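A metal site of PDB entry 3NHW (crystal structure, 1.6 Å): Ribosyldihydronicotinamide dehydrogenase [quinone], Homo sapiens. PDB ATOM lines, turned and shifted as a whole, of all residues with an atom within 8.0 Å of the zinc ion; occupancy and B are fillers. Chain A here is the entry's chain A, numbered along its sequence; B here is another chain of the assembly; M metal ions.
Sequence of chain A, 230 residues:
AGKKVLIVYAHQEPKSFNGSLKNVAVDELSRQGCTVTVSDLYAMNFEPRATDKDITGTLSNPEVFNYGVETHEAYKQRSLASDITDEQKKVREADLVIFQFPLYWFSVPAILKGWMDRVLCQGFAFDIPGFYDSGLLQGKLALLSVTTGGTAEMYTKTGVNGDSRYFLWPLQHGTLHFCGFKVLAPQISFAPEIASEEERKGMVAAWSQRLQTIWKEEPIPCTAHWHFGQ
N of His 177 sits at hydrogen-bond distance from O of Gln 172.
A ring nitrogen (NE2) of His 177 sits at hydrogen-bond distance from the side-chain carboxylate (OD1) of Asp 133, at 3.2 Å.
OH of Tyr 132 sits close to NE2 of His 173 (3.2 Å).
The backbone NH of Phe 178 sits at hydrogen-bond distance from the backbone carbonyl oxygen of His 173 (3.1 Å).
A ring nitrogen (NE2) of His 173 is in hydrogen-bond range of the backbone carbonyl oxygen (O) of Val 160 of chain B (3.2 Å).
O of Gln 172 lies close to SG of Cys 222 (3.5 Å).
O of Thr 223 lies within hydrogen-bond range of ND1 of His 227 (2.9 Å).
N of Trp 226 sits at hydrogen-bond distance from OG1 of Thr 223 (3.2 Å).
Thr 223 touches the zinc ion.
Within 4 Å of the zinc ion: His 173, His 177, Cys 222 and Thr 223.
Along chain A the residues within 4 Å of the zinc ion span positions 173 to 223.
The zinc ion is bound by a ring nitrogen (ND1) of His 177 (2.0 Å), a ring nitrogen (ND1) of His 173 (2.0 Å), the backbone carbonyl oxygen (O) of Cys 222 (2.1 Å) and the side-chain sulfur (SG) of Cys 222 (2.3 Å).
The zinc ion has four donor atoms within binding distance.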
ATOM      1  N   TYR A 132       7.841 -16.456 -13.419  1.00  0.00           N
ATOM      2  CA  TYR A 132       8.480 -15.169 -13.847  1.00  0.00           C
ATOM      3  C   TYR A 132       9.820 -15.046 -13.198  1.00  0.00           C
ATOM      4  O   TYR A 132      10.766 -15.739 -13.598  1.00  0.00           O
ATOM      5  CB  TYR A 132       7.659 -13.767 -13.728  1.00  0.00           C
ATOM      6  CG  TYR A 132       6.422 -13.707 -14.631  1.00  0.00           C
ATOM      7  CD1 TYR A 132       6.550 -13.538 -16.023  1.00  0.00           C
ATOM      8  CD2 TYR A 132       5.145 -13.916 -14.100  1.00  0.00           C
ATOM      9  CE1 TYR A 132       5.412 -13.581 -16.896  1.00  0.00           C
ATOM     10  CE2 TYR A 132       4.007 -13.969 -14.957  1.00  0.00           C
ATOM     11  CZ  TYR A 132       4.147 -13.834 -16.311  1.00  0.00           C
ATOM     12  OH  TYR A 132       3.016 -13.899 -17.069  1.00  0.00           O
ATOM     13  N   ASP A 133       9.959 -14.136 -12.238  1.00  0.00           N
ATOM     14  CA  ASP A 133      11.360 -13.964 -11.713  1.00  0.00           C
ATOM     15  C   ASP A 133      11.891 -15.067 -10.806  1.00  0.00           C
ATOM     16  O   ASP A 133      13.040 -15.260 -10.678  1.00  0.00           O
ATOM     17  CB  ASP A 133      11.637 -12.505 -11.286  1.00  0.00           C
ATOM     18  CG  ASP A 133      11.783 -11.631 -12.513  1.00  0.00           C
ATOM     19  OD1 ASP A 133      11.671 -12.224 -13.618  1.00  0.00           O
ATOM     20  OD2 ASP A 133      12.016 -10.413 -12.411  1.00  0.00           O
ATOM     21  N   TRP A 169       3.992 -11.295 -27.367  1.00  0.00           N
ATOM     22  CA  TRP A 169       3.662 -11.360 -25.954  1.00  0.00           C
ATOM     23  C   TRP A 169       3.501 -12.773 -25.366  1.00  0.00           C
ATOM     24  O   TRP A 169       4.146 -13.087 -24.374  1.00  0.00           O
ATOM     25  CB  TRP A 169       2.419 -10.425 -25.716  1.00  0.00           C
ATOM     26  CG  TRP A 169       1.830 -10.485 -24.378  1.00  0.00           C
ATOM     27  CD1 TRP A 169       0.623 -11.061 -24.004  1.00  0.00           C
ATOM     28  CD2 TRP A 169       2.325  -9.826 -23.192  1.00  0.00           C
ATOM     29  NE1 TRP A 169       0.393 -10.881 -22.642  1.00  0.00           N
ATOM     30  CE2 TRP A 169       1.393 -10.074 -22.151  1.00  0.00           C
ATOM     31  CE3 TRP A 169       3.477  -9.038 -22.927  1.00  0.00           C
ATOM     32  CZ2 TRP A 169       1.587  -9.574 -20.823  1.00  0.00           C
ATOM     33  CZ3 TRP A 169       3.655  -8.571 -21.643  1.00  0.00           C
ATOM     34  CH2 TRP A 169       2.725  -8.820 -20.638  1.00  0.00           C
ATOM     35  N   LEU A 171       4.732 -15.461 -26.442  1.00  0.00           N
ATOM     36  CA  LEU A 171       6.012 -16.201 -26.548  1.00  0.00           C
ATOM     37  C   LEU A 171       7.089 -15.644 -25.602  1.00  0.00           C
ATOM     38  O   LEU A 171       7.634 -16.413 -24.830  1.00  0.00           O
ATOM     39  CB  LEU A 171       6.534 -16.155 -27.953  1.00  0.00           C
ATOM     40  CG  LEU A 171       5.562 -16.870 -28.893  1.00  0.00           C
ATOM     41  CD1 LEU A 171       6.021 -16.550 -30.350  1.00  0.00           C
ATOM     42  CD2 LEU A 171       5.486 -18.419 -28.603  1.00  0.00           C
ATOM     43  N   GLN A 172       7.346 -14.376 -25.728  1.00  0.00           N
ATOM     44  CA  GLN A 172       8.378 -13.739 -24.861  1.00  0.00           C
ATOM     45  C   GLN A 172       7.938 -13.615 -23.411  1.00  0.00           C
ATOM     46  O   GLN A 172       8.691 -14.003 -22.432  1.00  0.00           O
ATOM     47  CB  GLN A 172       8.737 -12.406 -25.455  1.00  0.00           C
ATOM     48  CG  GLN A 172       9.389 -12.456 -26.851  1.00  0.00           C
ATOM     49  CD  GLN A 172       9.930 -11.179 -27.318  1.00  0.00           C
ATOM     50  OE1 GLN A 172       9.430 -10.078 -26.957  1.00  0.00           O
ATOM     51  NE2 GLN A 172      10.973 -11.258 -28.117  1.00  0.00           N
ATOM     52  N   HIS A 173       6.731 -13.064 -23.176  1.00  0.00           N
ATOM     53  CA  HIS A 173       6.310 -12.900 -21.785  1.00  0.00           C
ATOM     54  C   HIS A 173       5.696 -14.098 -21.173  1.00  0.00           C
ATOM     55  O   HIS A 173       6.123 -14.682 -20.132  1.00  0.00           O
ATOM     56  CB  HIS A 173       5.374 -11.664 -21.649  1.00  0.00           C
ATOM     57  CG  HIS A 173       5.047 -11.338 -20.218  1.00  0.00           C
ATOM     58  ND1 HIS A 173       5.928 -10.693 -19.354  1.00  0.00           N
ATOM     59  CD2 HIS A 173       3.937 -11.593 -19.484  1.00  0.00           C
ATOM     60  CE1 HIS A 173       5.357 -10.557 -18.177  1.00  0.00           C
ATOM     61  NE2 HIS A 173       4.153 -11.094 -18.227  1.00  0.00           N
ATOM     62  N   GLY A 174       4.677 -14.633 -21.860  1.00  0.00           N
ATOM     63  CA  GLY A 174       3.912 -15.706 -21.286  1.00  0.00           C
ATOM     64  C   GLY A 174       4.668 -17.051 -21.167  1.00  0.00           C
ATOM     65  O   GLY A 174       4.378 -17.842 -20.310  1.00  0.00           O
ATOM     66  N   THR A 175       5.678 -17.187 -22.013  1.00  0.00           N
ATOM     67  CA  THR A 175       6.448 -18.425 -22.005  1.00  0.00           C
ATOM     68  C   THR A 175       7.893 -18.170 -21.512  1.00  0.00           C
ATOM     69  O   THR A 175       8.211 -18.765 -20.475  1.00  0.00           O
ATOM     70  CB  THR A 175       6.491 -19.032 -23.440  1.00  0.00           C
ATOM     71  OG1 THR A 175       5.115 -19.174 -23.912  1.00  0.00           O
ATOM     72  CG2 THR A 175       7.014 -20.450 -23.362  1.00  0.00           C
ATOM     73  N   LEU A 176       8.687 -17.429 -22.269  1.00  0.00           N
ATOM     74  CA  LEU A 176      10.171 -17.313 -21.944  1.00  0.00           C
ATOM     75  C   LEU A 176      10.374 -16.613 -20.575  1.00  0.00           C
ATOM     76  O   LEU A 176      10.945 -17.190 -19.649  1.00  0.00           O
ATOM     77  CB  LEU A 176      10.912 -16.708 -23.101  1.00  0.00           C
ATOM     78  CG  LEU A 176      10.819 -17.501 -24.472  1.00  0.00           C
ATOM     79  CD1 LEU A 176      11.469 -16.691 -25.595  1.00  0.00           C
ATOM     80  CD2 LEU A 176      11.395 -18.898 -24.265  1.00  0.00           C
ATOM     81  N   HIS A 177       9.795 -15.431 -20.455  1.00  0.00           N
ATOM     82  CA  HIS A 177       9.895 -14.681 -19.147  1.00  0.00           C
ATOM     83  C   HIS A 177       9.365 -15.483 -18.033  1.00  0.00           C
ATOM     84  O   HIS A 177       9.947 -15.599 -16.953  1.00  0.00           O
ATOM     85  CB  HIS A 177       9.201 -13.336 -19.313  1.00  0.00           C
ATOM     86  CG  HIS A 177       9.439 -12.394 -18.136  1.00  0.00           C
ATOM     87  ND1 HIS A 177       8.984 -11.088 -18.154  1.00  0.00           N
ATOM     88  CD2 HIS A 177      10.053 -12.581 -16.935  1.00  0.00           C
ATOM     89  CE1 HIS A 177       9.336 -10.488 -17.014  1.00  0.00           C
ATOM     90  NE2 HIS A 177       9.972 -11.366 -16.241  1.00  0.00           N
ATOM     91  N   PHE A 178       8.167 -16.046 -18.193  1.00  0.00           N
ATOM     92  CA  PHE A 178       7.579 -16.820 -17.190  1.00  0.00           C
ATOM     93  C   PHE A 178       8.493 -17.907 -16.599  1.00  0.00           C
ATOM     94  O   PHE A 178       8.451 -18.157 -15.424  1.00  0.00           O
ATOM     95  CB  PHE A 178       6.284 -17.476 -17.735  1.00  0.00           C
ATOM     96  CG  PHE A 178       5.461 -18.128 -16.687  1.00  0.00           C
ATOM     97  CD1 PHE A 178       4.540 -17.309 -15.916  1.00  0.00           C
ATOM     98  CD2 PHE A 178       5.557 -19.488 -16.366  1.00  0.00           C
ATOM     99  CE1 PHE A 178       3.773 -17.887 -14.941  1.00  0.00           C
ATOM    100  CE2 PHE A 178       4.782 -20.083 -15.402  1.00  0.00           C
ATOM    101  CZ  PHE A 178       3.838 -19.233 -14.645  1.00  0.00           C
ATOM    102  N   PHE A 181      13.786 -16.992 -18.207  1.00  0.00           N
ATOM    103  CA  PHE A 181      14.654 -16.419 -19.175  1.00  0.00           C
ATOM    104  C   PHE A 181      14.708 -14.947 -19.230  1.00  0.00           C
ATOM    105  O   PHE A 181      13.685 -14.284 -19.083  1.00  0.00           O
ATOM    106  CB  PHE A 181      14.225 -16.827 -20.619  1.00  0.00           C
ATOM    107  CG  PHE A 181      14.397 -18.303 -20.935  1.00  0.00           C
ATOM    108  CD1 PHE A 181      15.656 -18.773 -21.403  1.00  0.00           C
ATOM    109  CD2 PHE A 181      13.331 -19.221 -20.764  1.00  0.00           C
ATOM    110  CE1 PHE A 181      15.809 -20.154 -21.742  1.00  0.00           C
ATOM    111  CE2 PHE A 181      13.492 -20.585 -21.070  1.00  0.00           C
ATOM    112  CZ  PHE A 181      14.780 -21.027 -21.580  1.00  0.00           C
ATOM    113  N   VAL A 183      15.183 -12.257 -21.986  1.00  0.00           N
ATOM    114  CA  VAL A 183      14.818 -12.275 -23.401  1.00  0.00           C
ATOM    115  C   VAL A 183      15.589 -11.268 -24.228  1.00  0.00           C
ATOM    116  O   VAL A 183      15.504 -10.010 -24.060  1.00  0.00           O
ATOM    117  CB  VAL A 183      13.222 -12.126 -23.583  1.00  0.00           C
ATOM    118  CG1 VAL A 183      12.839 -12.046 -25.043  1.00  0.00           C
ATOM    119  CG2 VAL A 183      12.474 -13.083 -22.679  1.00  0.00           C
ATOM    120  N   ILE A 220      15.927  -7.341 -23.324  1.00  0.00           N
ATOM    121  CA  ILE A 220      14.801  -6.348 -23.405  1.00  0.00           C
ATOM    122  C   ILE A 220      14.101  -6.296 -22.077  1.00  0.00           C
ATOM    123  O   ILE A 220      14.158  -7.209 -21.302  1.00  0.00           O
ATOM    124  CB  ILE A 220      13.701  -6.727 -24.452  1.00  0.00           C
ATOM    125  CG1 ILE A 220      12.912  -8.009 -24.042  1.00  0.00           C
ATOM    126  CG2 ILE A 220      14.253  -6.701 -25.799  1.00  0.00           C
ATOM    127  CD1 ILE A 220      11.546  -8.218 -24.861  1.00  0.00           C
ATOM    128  N   PRO A 221      13.400  -5.177 -21.747  1.00  0.00           N
ATOM    129  CA  PRO A 221      12.700  -5.414 -20.469  1.00  0.00           C
ATOM    130  C   PRO A 221      11.346  -6.074 -20.769  1.00  0.00           C
ATOM    131  O   PRO A 221      10.582  -5.463 -21.481  1.00  0.00           O
ATOM    132  CB  PRO A 221      12.464  -3.982 -19.944  1.00  0.00           C
ATOM    133  CG  PRO A 221      12.431  -3.131 -21.169  1.00  0.00           C
ATOM    134  CD  PRO A 221      13.242  -3.822 -22.283  1.00  0.00           C
ATOM    135  N   CYS A 222      11.075  -7.259 -20.226  1.00  0.00           N
ATOM    136  CA  CYS A 222      10.001  -8.102 -20.808  1.00  0.00           C
ATOM    137  C   CYS A 222       8.681  -7.728 -20.080  1.00  0.00           C
ATOM    138  O   CYS A 222       8.244  -8.379 -19.134  1.00  0.00           O
ATOM    139  CB  CYS A 222      10.360  -9.593 -20.738  1.00  0.00           C
ATOM    140  SG  CYS A 222       9.010 -10.575 -21.624  1.00  0.00           S
ATOM    141  N   THR A 223       8.147  -6.593 -20.485  1.00  0.00           N
ATOM    142  CA  THR A 223       7.003  -6.053 -19.764  1.00  0.00           C
ATOM    143  C   THR A 223       5.894  -5.720 -20.759  1.00  0.00           C
ATOM    144  O   THR A 223       6.112  -5.514 -21.965  1.00  0.00           O
ATOM    145  CB  THR A 223       7.361  -4.722 -19.019  1.00  0.00           C
ATOM    146  OG1 THR A 223       7.828  -3.830 -20.005  1.00  0.00           O
ATOM    147  CG2 THR A 223       8.424  -4.923 -17.941  1.00  0.00           C
ATOM    148  N   ALA A 224       4.686  -5.599 -20.213  1.00  0.00           N
ATOM    149  CA  ALA A 224       3.583  -5.105 -20.991  1.00  0.00           C
ATOM    150  C   ALA A 224       3.891  -3.803 -21.733  1.00  0.00           C
ATOM    151  O   ALA A 224       3.559  -3.636 -22.905  1.00  0.00           O
ATOM    152  CB  ALA A 224       2.262  -5.011 -20.060  1.00  0.00           C
ATOM    153  N   TRP A 226       6.841  -2.671 -22.785  1.00  0.00           N
ATOM    154  CA  TRP A 226       7.639  -2.968 -23.984  1.00  0.00           C
ATOM    155  C   TRP A 226       6.773  -3.402 -25.223  1.00  0.00           C
ATOM    156  O   TRP A 226       6.967  -2.968 -26.381  1.00  0.00           O
ATOM    157  CB  TRP A 226       8.683  -4.073 -23.606  1.00  0.00           C
ATOM    158  CG  TRP A 226       9.727  -4.243 -24.696  1.00  0.00           C
ATOM    159  CD1 TRP A 226      10.870  -3.523 -24.837  1.00  0.00           C
ATOM    160  CD2 TRP A 226       9.664  -5.139 -25.836  1.00  0.00           C
ATOM    161  NE1 TRP A 226      11.522  -3.890 -25.971  1.00  0.00           N
ATOM    162  CE2 TRP A 226      10.818  -4.903 -26.607  1.00  0.00           C
ATOM    163  CE3 TRP A 226       8.748  -6.115 -26.269  1.00  0.00           C
ATOM    164  CZ2 TRP A 226      11.102  -5.616 -27.806  1.00  0.00           C
ATOM    165  CZ3 TRP A 226       9.009  -6.788 -27.478  1.00  0.00           C
ATOM    166  CH2 TRP A 226      10.172  -6.558 -28.217  1.00  0.00           C
ATOM    167  N   HIS A 227       5.812  -4.294 -24.979  1.00  0.00           N
ATOM    168  CA  HIS A 227       5.120  -4.927 -26.074  1.00  0.00           C
ATOM    169  C   HIS A 227       3.996  -4.073 -26.653  1.00  0.00           C
ATOM    170  O   HIS A 227       3.789  -4.049 -27.856  1.00  0.00           O
ATOM    171  CB  HIS A 227       4.528  -6.292 -25.625  1.00  0.00           C
ATOM    172  CG  HIS A 227       5.571  -7.350 -25.323  1.00  0.00           C
ATOM    173  ND1 HIS A 227       6.217  -7.455 -24.096  1.00  0.00           N
ATOM    174  CD2 HIS A 227       5.982  -8.416 -26.061  1.00  0.00           C
ATOM    175  CE1 HIS A 227       7.003  -8.531 -24.118  1.00  0.00           C
ATOM    176  NE2 HIS A 227       6.892  -9.108 -25.307  1.00  0.00           N
ATOM    177  N   VAL B 160       0.284 -10.064 -12.716  1.00  0.00           N
ATOM    178  CA  VAL B 160       1.527 -10.656 -13.259  1.00  0.00           C
ATOM    179  C   VAL B 160       1.420 -11.065 -14.698  1.00  0.00           C
ATOM    180  O   VAL B 160       2.414 -10.926 -15.513  1.00  0.00           O
ATOM    181  CB  VAL B 160       2.005 -11.877 -12.495  1.00  0.00           C
ATOM    182  CG1 VAL B 160       2.820 -11.429 -11.270  1.00  0.00           C
ATOM    183  CG2 VAL B 160       0.878 -12.841 -12.187  1.00  0.00           C
HETATM  184 ZN    ZN M   1       7.895 -10.434 -19.645  1.00  0.00          ZN
